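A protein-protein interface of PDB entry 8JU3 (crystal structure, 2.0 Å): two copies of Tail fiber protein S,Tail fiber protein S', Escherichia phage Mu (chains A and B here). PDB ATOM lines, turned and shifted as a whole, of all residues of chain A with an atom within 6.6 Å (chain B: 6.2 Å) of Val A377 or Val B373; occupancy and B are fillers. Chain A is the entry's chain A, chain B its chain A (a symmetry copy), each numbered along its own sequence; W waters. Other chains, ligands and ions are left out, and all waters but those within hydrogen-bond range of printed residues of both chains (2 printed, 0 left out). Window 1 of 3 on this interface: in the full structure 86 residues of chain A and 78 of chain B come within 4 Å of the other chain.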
ATOM      1  N   VAL A 348     -19.496  17.462  25.618  1.00  0.00           N
ATOM      2  CA  VAL A 348     -20.898  17.844  25.712  1.00  0.00           C
ATOM      3  C   VAL A 348     -21.419  17.255  27.023  1.00  0.00           C
ATOM      4  O   VAL A 348     -21.436  16.035  27.197  1.00  0.00           O
ATOM      5  CB  VAL A 348     -21.728  17.301  24.518  1.00  0.00           C
ATOM      6  CG1 VAL A 348     -23.224  17.882  24.566  1.00  0.00           C
ATOM      7  CG2 VAL A 348     -21.088  17.678  23.180  1.00  0.00           C
ATOM      8  N   SER A 357     -33.317  19.775  32.423  1.00  0.00           N
ATOM      9  CA  SER A 357     -31.855  19.847  32.380  1.00  0.00           C
ATOM     10  C   SER A 357     -31.493  20.680  31.169  1.00  0.00           C
ATOM     11  O   SER A 357     -32.364  21.078  30.392  1.00  0.00           O
ATOM     12  CB  SER A 357     -31.226  18.441  32.291  1.00  0.00           C
ATOM     13  OG  SER A 357     -31.421  17.872  30.978  1.00  0.00           O
ATOM     14  N   THR A 358     -30.218  21.022  31.044  1.00  0.00           N
ATOM     15  CA  THR A 358     -29.785  21.920  29.991  1.00  0.00           C
ATOM     16  C   THR A 358     -28.451  21.366  29.427  1.00  0.00           C
ATOM     17  O   THR A 358     -27.755  20.564  30.079  1.00  0.00           O
ATOM     18  CB  THR A 358     -29.631  23.381  30.500  1.00  0.00           C
ATOM     19  OG1 THR A 358     -29.365  24.245  29.406  1.00  0.00           O
ATOM     20  CG2 THR A 358     -28.288  23.510  31.427  1.00  0.00           C
ATOM     21  N   LEU A 359     -28.087  21.798  28.221  1.00  0.00           N
ATOM     22  CA  LEU A 359     -26.908  21.277  27.537  1.00  0.00           C
ATOM     23  C   LEU A 359     -25.746  22.228  27.781  1.00  0.00           C
ATOM     24  O   LEU A 359     -25.883  23.437  27.575  1.00  0.00           O
ATOM     25  CB  LEU A 359     -27.160  21.176  26.014  1.00  0.00           C
ATOM     26  CG  LEU A 359     -25.980  20.581  25.150  1.00  0.00           C
ATOM     27  CD1 LEU A 359     -26.491  19.817  23.889  1.00  0.00           C
ATOM     28  CD2 LEU A 359     -25.069  21.731  24.641  1.00  0.00           C
ATOM     29  N   ILE A 360     -24.585  21.699  28.167  1.00  0.00           N
ATOM     30  CA  ILE A 360     -23.388  22.541  28.396  1.00  0.00           C
ATOM     31  C   ILE A 360     -22.323  22.089  27.404  1.00  0.00           C
ATOM     32  O   ILE A 360     -21.926  20.922  27.423  1.00  0.00           O
ATOM     33  CB  ILE A 360     -22.867  22.398  29.843  1.00  0.00           C
ATOM     34  CG1 ILE A 360     -23.889  22.809  30.881  1.00  0.00           C
ATOM     35  CG2 ILE A 360     -21.581  23.321  30.021  1.00  0.00           C
ATOM     36  CD1 ILE A 360     -24.363  24.261  30.712  1.00  0.00           C
ATOM     37  N   LEU A 361     -21.879  22.978  26.516  1.00  0.00           N
ATOM     38  CA  LEU A 361     -20.882  22.587  25.539  1.00  0.00           C
ATOM     39  C   LEU A 361     -19.599  23.232  26.033  1.00  0.00           C
ATOM     40  O   LEU A 361     -19.571  24.448  26.202  1.00  0.00           O
ATOM     41  CB  LEU A 361     -21.338  23.077  24.151  1.00  0.00           C
ATOM     42  CG  LEU A 361     -20.302  23.039  23.041  1.00  0.00           C
ATOM     43  CD1 LEU A 361     -19.971  21.514  22.743  1.00  0.00           C
ATOM     44  CD2 LEU A 361     -20.938  23.629  21.737  1.00  0.00           C
ATOM     45  N   PHE A 375     -20.776  27.003  26.514  1.00  0.00           N
ATOM     46  CA  PHE A 375     -22.045  27.504  26.013  1.00  0.00           C
ATOM     47  C   PHE A 375     -23.128  26.801  26.792  1.00  0.00           C
ATOM     48  O   PHE A 375     -23.068  25.581  26.964  1.00  0.00           O
ATOM     49  CB  PHE A 375     -22.257  27.182  24.544  1.00  0.00           C
ATOM     50  CG  PHE A 375     -21.248  27.819  23.651  1.00  0.00           C
ATOM     51  CD1 PHE A 375     -20.031  27.199  23.399  1.00  0.00           C
ATOM     52  CD2 PHE A 375     -21.525  29.056  23.053  1.00  0.00           C
ATOM     53  CE1 PHE A 375     -19.096  27.803  22.587  1.00  0.00           C
ATOM     54  CE2 PHE A 375     -20.571  29.659  22.213  1.00  0.00           C
ATOM     55  CZ  PHE A 375     -19.364  29.049  21.998  1.00  0.00           C
ATOM     56  N   ARG A 376     -24.157  27.515  27.181  1.00  0.00           N
ATOM     57  CA  ARG A 376     -25.320  26.828  27.763  1.00  0.00           C
ATOM     58  C   ARG A 376     -26.426  26.906  26.712  1.00  0.00           C
ATOM     59  O   ARG A 376     -26.632  27.979  26.118  1.00  0.00           O
ATOM     60  CB  ARG A 376     -25.806  27.502  29.035  1.00  0.00           C
ATOM     61  CG  ARG A 376     -27.220  26.959  29.449  1.00  0.00           C
ATOM     62  CD  ARG A 376     -27.838  27.690  30.707  1.00  0.00           C
ATOM     63  NE  ARG A 376     -29.219  27.188  30.890  1.00  0.00           N
ATOM     64  CZ  ARG A 376     -29.919  27.201  32.021  1.00  0.00           C
ATOM     65  NH1 ARG A 376     -29.370  27.548  33.169  1.00  0.00           N
ATOM     66  NH2 ARG A 376     -31.205  26.824  32.005  1.00  0.00           N
ATOM     67  N   VAL A 377     -27.086  25.779  26.440  1.00  0.00           N
ATOM     68  CA  VAL A 377     -28.125  25.731  25.425  1.00  0.00           C
ATOM     69  C   VAL A 377     -29.396  25.147  26.055  1.00  0.00           C
ATOM     70  O   VAL A 377     -29.391  23.991  26.509  1.00  0.00           O
ATOM     71  CB  VAL A 377     -27.685  24.892  24.211  1.00  0.00           C
ATOM     72  CG1 VAL A 377     -28.811  25.039  23.068  1.00  0.00           C
ATOM     73  CG2 VAL A 377     -26.304  25.306  23.627  1.00  0.00           C
ATOM     74  N   ASN A 378     -30.505  25.908  26.016  1.00  0.00           N
ATOM     75  CA  ASN A 378     -31.802  25.434  26.556  1.00  0.00           C
ATOM     76  C   ASN A 378     -32.617  24.709  25.484  1.00  0.00           C
ATOM     77  O   ASN A 378     -32.554  25.072  24.314  1.00  0.00           O
ATOM     78  CB  ASN A 378     -32.650  26.635  27.062  1.00  0.00           C
ATOM     79  CG  ASN A 378     -32.056  27.296  28.287  1.00  0.00           C
ATOM     80  OD1 ASN A 378     -31.319  26.631  29.098  1.00  0.00           O
ATOM     81  ND2 ASN A 378     -32.451  28.583  28.519  1.00  0.00           N
ATOM     82  N   TYR A 379     -33.489  23.773  25.902  1.00  0.00           N
ATOM     83  CA  TYR A 379     -34.154  22.955  24.886  1.00  0.00           C
ATOM     84  C   TYR A 379     -35.091  23.798  24.021  1.00  0.00           C
ATOM     85  O   TYR A 379     -35.575  24.844  24.454  1.00  0.00           O
ATOM     86  CB  TYR A 379     -34.924  21.812  25.538  1.00  0.00           C
ATOM     87  CG  TYR A 379     -36.036  22.279  26.464  1.00  0.00           C
ATOM     88  CD1 TYR A 379     -37.306  22.594  25.957  1.00  0.00           C
ATOM     89  CD2 TYR A 379     -35.844  22.363  27.849  1.00  0.00           C
ATOM     90  CE1 TYR A 379     -38.342  22.980  26.796  1.00  0.00           C
ATOM     91  CE2 TYR A 379     -36.922  22.775  28.731  1.00  0.00           C
ATOM     92  CZ  TYR A 379     -38.147  23.075  28.171  1.00  0.00           C
ATOM     93  OH  TYR A 379     -39.206  23.450  28.971  1.00  0.00           O
ATOM     94  N   ASN A 381     -34.731  25.792  21.260  1.00  0.00           N
ATOM     95  CA  ASN A 381     -34.290  27.181  21.075  1.00  0.00           C
ATOM     96  C   ASN A 381     -34.708  28.051  22.266  1.00  0.00           C
ATOM     97  O   ASN A 381     -35.146  29.211  22.103  1.00  0.00           O
ATOM     98  CB  ASN A 381     -34.823  27.796  19.728  1.00  0.00           C
ATOM     99  CG  ASN A 381     -34.272  27.107  18.478  1.00  0.00           C
ATOM    100  OD1 ASN A 381     -34.134  25.873  18.426  1.00  0.00           O
ATOM    101  ND2 ASN A 381     -33.984  27.930  17.412  1.00  0.00           N
ATOM    102  N   GLY A 382     -34.531  27.523  23.484  1.00  0.00           N
ATOM    103  CA  GLY A 382     -34.948  28.272  24.654  1.00  0.00           C
ATOM    104  C   GLY A 382     -33.935  29.284  25.119  1.00  0.00           C
ATOM    105  O   GLY A 382     -34.087  29.874  26.195  1.00  0.00           O
ATOM    106  N   GLY A 383     -32.871  29.478  24.362  1.00  0.00           N
ATOM    107  CA  GLY A 383     -31.854  30.442  24.775  1.00  0.00           C
ATOM    108  C   GLY A 383     -30.454  29.826  24.634  1.00  0.00           C
ATOM    109  O   GLY A 383     -30.298  28.614  24.828  1.00  0.00           O
ATOM    110  N   ILE A 384     -29.464  30.605  24.215  1.00  0.00           N
ATOM    111  CA  ILE A 384     -28.079  30.145  24.136  1.00  0.00           C
ATOM    112  C   ILE A 384     -27.202  31.245  24.770  1.00  0.00           C
ATOM    113  O   ILE A 384     -27.475  32.438  24.615  1.00  0.00           O
ATOM    114  CB  ILE A 384     -27.654  29.826  22.679  1.00  0.00           C
ATOM    115  CG1 ILE A 384     -26.182  29.337  22.622  1.00  0.00           C
ATOM    116  CG2 ILE A 384     -27.769  31.051  21.711  1.00  0.00           C
ATOM    117  CD1 ILE A 384     -25.848  28.805  21.244  1.00  0.00           C
ATOM    118  N   PHE A 385     -26.223  30.835  25.565  1.00  0.00           N
ATOM    119  CA  PHE A 385     -25.429  31.711  26.445  1.00  0.00           C
ATOM    120  C   PHE A 385     -23.969  31.256  26.393  1.00  0.00           C
ATOM    121  O   PHE A 385     -23.709  30.116  26.044  1.00  0.00           O
ATOM    122  CB  PHE A 385     -25.823  31.627  27.903  1.00  0.00           C
ATOM    123  CG  PHE A 385     -27.340  31.598  28.211  1.00  0.00           C
ATOM    124  CD1 PHE A 385     -28.148  30.503  27.879  1.00  0.00           C
ATOM    125  CD2 PHE A 385     -27.900  32.656  28.914  1.00  0.00           C
ATOM    126  CE1 PHE A 385     -29.483  30.545  28.159  1.00  0.00           C
ATOM    127  CE2 PHE A 385     -29.220  32.700  29.233  1.00  0.00           C
ATOM    128  CZ  PHE A 385     -30.036  31.619  28.835  1.00  0.00           C
ATOM    129  N   LEU B 361     -22.751  22.566  12.320  1.00  0.00           N
ATOM    130  CA  LEU B 361     -21.895  22.084  13.386  1.00  0.00           C
ATOM    131  C   LEU B 361     -22.853  21.452  14.380  1.00  0.00           C
ATOM    132  O   LEU B 361     -23.762  22.134  14.844  1.00  0.00           O
ATOM    133  CB  LEU B 361     -21.098  23.274  13.950  1.00  0.00           C
ATOM    134  CG  LEU B 361     -20.371  23.045  15.265  1.00  0.00           C
ATOM    135  CD1 LEU B 361     -19.213  21.990  14.999  1.00  0.00           C
ATOM    136  CD2 LEU B 361     -19.676  24.382  15.696  1.00  0.00           C
ATOM    137  N   HIS B 362     -22.764  20.127  14.591  1.00  0.00           N
ATOM    138  CA  HIS B 362     -23.778  19.376  15.315  1.00  0.00           C
ATOM    139  C   HIS B 362     -23.137  18.764  16.557  1.00  0.00           C
ATOM    140  O   HIS B 362     -22.089  18.129  16.443  1.00  0.00           O
ATOM    141  CB  HIS B 362     -24.315  18.243  14.386  1.00  0.00           C
ATOM    142  CG  HIS B 362     -25.205  17.276  15.069  1.00  0.00           C
ATOM    143  ND1 HIS B 362     -26.462  17.656  15.549  1.00  0.00           N
ATOM    144  CD2 HIS B 362     -25.092  15.938  15.295  1.00  0.00           C
ATOM    145  CE1 HIS B 362     -27.057  16.593  16.076  1.00  0.00           C
ATOM    146  NE2 HIS B 362     -26.233  15.549  15.975  1.00  0.00           N
ATOM    147  N   PHE B 363     -23.765  18.938  17.729  1.00  0.00           N
ATOM    148  CA  PHE B 363     -23.388  18.281  18.979  1.00  0.00           C
ATOM    149  C   PHE B 363     -24.591  17.527  19.530  1.00  0.00           C
ATOM    150  O   PHE B 363     -25.645  18.135  19.730  1.00  0.00           O
ATOM    151  CB  PHE B 363     -22.955  19.361  19.993  1.00  0.00           C
ATOM    152  CG  PHE B 363     -21.678  20.092  19.539  1.00  0.00           C
ATOM    153  CD1 PHE B 363     -20.431  19.475  19.692  1.00  0.00           C
ATOM    154  CD2 PHE B 363     -21.763  21.304  18.885  1.00  0.00           C
ATOM    155  CE1 PHE B 363     -19.221  20.155  19.217  1.00  0.00           C
ATOM    156  CE2 PHE B 363     -20.608  21.999  18.481  1.00  0.00           C
ATOM    157  CZ  PHE B 363     -19.336  21.366  18.576  1.00  0.00           C
ATOM    158  N   ASN B 364     -24.397  16.293  19.923  1.00  0.00           N
ATOM    159  CA  ASN B 364     -25.481  15.460  20.420  1.00  0.00           C
ATOM    160  C   ASN B 364     -24.906  14.591  21.526  1.00  0.00           C
ATOM    161  O   ASN B 364     -23.871  13.938  21.329  1.00  0.00           O
ATOM    162  CB  ASN B 364     -26.063  14.596  19.287  1.00  0.00           C
ATOM    163  CG  ASN B 364     -26.860  13.446  19.828  1.00  0.00           C
ATOM    164  OD1 ASN B 364     -27.647  13.641  20.771  1.00  0.00           O
ATOM    165  ND2 ASN B 364     -26.629  12.245  19.334  1.00  0.00           N
ATOM    166  N   CYS B 370     -32.363  18.847  26.669  1.00  0.00           N
ATOM    167  CA  CYS B 370     -31.826  19.331  25.397  1.00  0.00           C
ATOM    168  C   CYS B 370     -30.671  18.404  25.034  1.00  0.00           C
ATOM    169  O   CYS B 370     -29.546  18.609  25.524  1.00  0.00           O
ATOM    170  CB  CYS B 370     -31.334  20.814  25.485  1.00  0.00           C
ATOM    171  SG  CYS B 370     -30.630  21.386  23.900  1.00  0.00           S
ATOM    172  N   PRO B 371     -30.873  17.392  24.177  1.00  0.00           N
ATOM    173  CA  PRO B 371     -29.774  16.436  23.891  1.00  0.00           C
ATOM    174  C   PRO B 371     -28.834  16.927  22.788  1.00  0.00           C
ATOM    175  O   PRO B 371     -27.751  16.358  22.630  1.00  0.00           O
ATOM    176  CB  PRO B 371     -30.524  15.140  23.454  1.00  0.00           C
ATOM    177  CG  PRO B 371     -31.868  15.698  22.727  1.00  0.00           C
ATOM    178  CD  PRO B 371     -32.184  16.959  23.658  1.00  0.00           C
ATOM    179  N   ALA B 372     -29.172  17.996  22.066  1.00  0.00           N
ATOM    180  CA  ALA B 372     -28.429  18.323  20.868  1.00  0.00           C
ATOM    181  C   ALA B 372     -28.580  19.790  20.535  1.00  0.00           C
ATOM    182  O   ALA B 372     -29.599  20.426  20.792  1.00  0.00           O
ATOM    183  CB  ALA B 372     -28.890  17.450  19.651  1.00  0.00           C
ATOM    184  N   VAL B 373     -27.554  20.328  19.937  1.00  0.00           N
ATOM    185  CA  VAL B 373     -27.624  21.681  19.414  1.00  0.00           C
ATOM    186  C   VAL B 373     -26.908  21.672  18.073  1.00  0.00           C
ATOM    187  O   VAL B 373     -25.908  20.969  17.885  1.00  0.00           O
ATOM    188  CB  VAL B 373     -26.969  22.718  20.394  1.00  0.00           C
ATOM    189  CG1 VAL B 373     -25.426  22.413  20.669  1.00  0.00           C
ATOM    190  CG2 VAL B 373     -26.998  24.176  19.804  1.00  0.00           C
ATOM    191  N   GLN B 374     -27.404  22.472  17.129  1.00  0.00           N
ATOM    192  CA  GLN B 374     -26.744  22.609  15.843  1.00  0.00           C
ATOM    193  C   GLN B 374     -26.579  24.076  15.563  1.00  0.00           C
ATOM    194  O   GLN B 374     -27.430  24.892  15.940  1.00  0.00           O
ATOM    195  CB  GLN B 374     -27.551  22.017  14.652  1.00  0.00           C
ATOM    196  CG  GLN B 374     -27.790  20.641  14.827  1.00  0.00           C
ATOM    197  CD  GLN B 374     -28.514  19.929  13.638  1.00  0.00           C
ATOM    198  OE1 GLN B 374     -29.142  20.551  12.795  1.00  0.00           O
ATOM    199  NE2 GLN B 374     -28.461  18.597  13.652  1.00  0.00           N
ATOM    200  N   PHE B 375     -25.472  24.404  14.895  1.00  0.00           N
ATOM    201  CA  PHE B 375     -25.244  25.755  14.413  1.00  0.00           C
ATOM    202  C   PHE B 375     -25.237  25.684  12.907  1.00  0.00           C
ATOM    203  O   PHE B 375     -24.596  24.799  12.335  1.00  0.00           O
ATOM    204  CB  PHE B 375     -23.898  26.307  14.849  1.00  0.00           C
ATOM    205  CG  PHE B 375     -23.764  26.433  16.327  1.00  0.00           C
ATOM    206  CD1 PHE B 375     -23.340  25.356  17.097  1.00  0.00           C
ATOM    207  CD2 PHE B 375     -24.066  27.648  16.955  1.00  0.00           C
ATOM    208  CE1 PHE B 375     -23.236  25.475  18.465  1.00  0.00           C
ATOM    209  CE2 PHE B 375     -23.944  27.766  18.353  1.00  0.00           C
ATOM    210  CZ  PHE B 375     -23.552  26.687  19.100  1.00  0.00           C
ATOM    211  N   TYR B 386     -28.631  29.022  15.356  1.00  0.00           N
ATOM    212  CA  TYR B 386     -28.627  27.772  16.090  1.00  0.00           C
ATOM    213  C   TYR B 386     -30.040  27.218  16.181  1.00  0.00           C
ATOM    214  O   TYR B 386     -31.045  27.923  15.956  1.00  0.00           O
ATOM    215  CB  TYR B 386     -27.966  27.930  17.487  1.00  0.00           C
ATOM    216  CG  TYR B 386     -28.989  28.364  18.580  1.00  0.00           C
ATOM    217  CD1 TYR B 386     -29.557  29.656  18.573  1.00  0.00           C
ATOM    218  CD2 TYR B 386     -29.440  27.451  19.539  1.00  0.00           C
ATOM    219  CE1 TYR B 386     -30.554  30.022  19.517  1.00  0.00           C
ATOM    220  CE2 TYR B 386     -30.399  27.824  20.580  1.00  0.00           C
ATOM    221  CZ  TYR B 386     -30.947  29.151  20.518  1.00  0.00           C
ATOM    222  OH  TYR B 386     -31.877  29.538  21.483  1.00  0.00           O
ATOM    223  N   ARG B 387     -30.113  25.901  16.451  1.00  0.00           N
ATOM    224  CA  ARG B 387     -31.381  25.338  16.874  1.00  0.00           C
ATOM    225  C   ARG B 387     -31.064  24.209  17.845  1.00  0.00           C
ATOM    226  O   ARG B 387     -29.980  23.624  17.784  1.00  0.00           O
ATOM    227  CB  ARG B 387     -32.191  24.795  15.689  1.00  0.00           C
ATOM    228  CG  ARG B 387     -31.527  23.653  14.927  1.00  0.00           C
ATOM    229  CD  ARG B 387     -32.460  23.236  13.739  1.00  0.00           C
ATOM    230  NE  ARG B 387     -31.895  22.077  13.049  1.00  0.00           N
ATOM    231  CZ  ARG B 387     -32.588  21.214  12.343  1.00  0.00           C
ATOM    232  NH1 ARG B 387     -33.906  21.356  12.207  1.00  0.00           N
ATOM    233  NH2 ARG B 387     -31.947  20.174  11.777  1.00  0.00           N
ATOM    234  N   SER B 388     -31.990  23.924  18.775  1.00  0.00           N
ATOM    235  CA  SER B 388     -31.630  22.967  19.814  1.00  0.00           C
ATOM    236  C   SER B 388     -32.822  22.054  20.051  1.00  0.00           C
ATOM    237  O   SER B 388     -33.990  22.467  19.936  1.00  0.00           O
ATOM    238  CB  SER B 388     -31.199  23.694  21.102  1.00  0.00           C
ATOM    239  OG  SER B 388     -32.334  24.455  21.664  1.00  0.00           O
ATOM    240  N   ALA B 389     -32.538  20.843  20.465  1.00  0.00           N
ATOM    241  CA  ALA B 389     -33.576  19.831  20.447  1.00  0.00           C
ATOM    242  C   ALA B 389     -34.276  19.794  21.804  1.00  0.00           C
ATOM    243  O   ALA B 389     -33.945  20.566  22.720  1.00  0.00           O
ATOM    244  CB  ALA B 389     -33.015  18.436  20.119  1.00  0.00           C
ATOM    245  N   PHE B 395     -35.858  18.969  16.723  1.00  0.00           N
ATOM    246  CA  PHE B 395     -35.765  20.409  16.655  1.00  0.00           C
ATOM    247  C   PHE B 395     -37.128  20.951  16.240  1.00  0.00           C
ATOM    248  O   PHE B 395     -37.394  21.058  15.056  1.00  0.00           O
ATOM    249  CB  PHE B 395     -34.711  20.835  15.612  1.00  0.00           C
ATOM    250  CG  PHE B 395     -33.320  20.261  15.876  1.00  0.00           C
ATOM    251  CD1 PHE B 395     -32.828  19.212  15.106  1.00  0.00           C
ATOM    252  CD2 PHE B 395     -32.565  20.740  16.951  1.00  0.00           C
ATOM    253  CE1 PHE B 395     -31.562  18.685  15.364  1.00  0.00           C
ATOM    254  CE2 PHE B 395     -31.239  20.274  17.225  1.00  0.00           C
ATOM    255  CZ  PHE B 395     -30.730  19.260  16.440  1.00  0.00           C
HETATM  256  O   HOH W   1     -29.993  18.852  28.271  1.00  0.00           O
HETATM  257  O   HOH W   2     -35.594  23.601  17.787  1.00  0.00           O
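The side-chain hydroxyl (OG) of Ser B388 sits at hydrogen-bond distance from the backbone carbonyl oxygen (O) of Asn A378 (2.7 Å). The side-chain amide nitrogen (ND2) of Asn A381 is in hydrogen-bond range of the backbone carbonyl oxygen (O) of Tyr B386, at 3.3 Å. OG of Ser B388 sits at hydrogen-bond distance from N of Asn A381. The backbone NH (N) of Gly A383 lies within hydrogen-bond range of the side-chain hydroxyl (OH) of Tyr B386.
The side-chain hydroxyl of Thr A358 lies within hydrogen-bond range of the backbone carbonyl oxygen of Val A377 (2.9 Å). The backbone carbonyl oxygen of Leu A361 sits at hydrogen-bond distance from the backbone NH of Phe A375 (2.8 Å). O of Gly A382 is in hydrogen-bond range of ND2 of Asn A378 (3.1 Å). O of Gly A383 sits at hydrogen-bond distance from N of Asn A378 (3.0 Å). The backbone NH (N) of Phe B375 sits at hydrogen-bond distance from the backbone carbonyl oxygen (O) of Leu B361, 2.8 Å away. The backbone carbonyl oxygen (O) of Ala B372 is in hydrogen-bond range of the backbone NH (N) of Ala B389 (3.0 Å).
CG2 of Val A348 touches CD1 of Phe B363, 3.98 Å away. Phe B363 touches Leu A361 (CE2 to CD2, 3.7 Å). Val A377 touches Ser B388. Tyr A379 touches Cys B370 (CA to CB, 3.6 Å). Tyr A379 touches Ser B388. O of Ala B389 touches CA of Tyr A379, at 3.2 Å. Arg B387 touches Asn A381. OH of Tyr B386 touches N of Gly A382 (3.9 Å). Ile A384 touches Phe B375 (CD1 to CE2, 3.6 Å). CG2 of Ile A384 touches CE1 of Tyr B386 (3.7 Å).
Of the printed residues of chain B, Leu A361 touches Phe B363. Val A377 touches three residues of chain B. Of the printed residues of chain B, Asn A378 touches Ser B388. Of chain A, only Val A377 comes within 4 Å of Val B373. The nearest printed residue of chain B that does not touch Gly A383 is Ser B388 (5.6 Å).
Hydrophobic or aromatic side chains of chain A that line the printed part of chain B: Val A348, Leu A359, Leu A361, Val A377, Tyr A379 and Ile A384. Hydrophobic or aromatic side chains of chain B within 4 Å of the printed part of chain A: Phe B363, Val B373, Phe B375 and Tyr B386. Among the printed residues, no Asp or Glu carboxylate lies within 4 Å of a Lys or Arg side-chain nitrogen of the other chain.
Positions printed for both chains: 361 and 375.
Water W2 bridges OD1 of Asn A381 (2.8 Å) and O of Ser B388 (2.9 Å). Water W1 lies within hydrogen-bond range of O of Cys B370 (2.8 Å), OG of Ser A357 (3.2 Å) and O of Thr A358 (3.3 Å).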
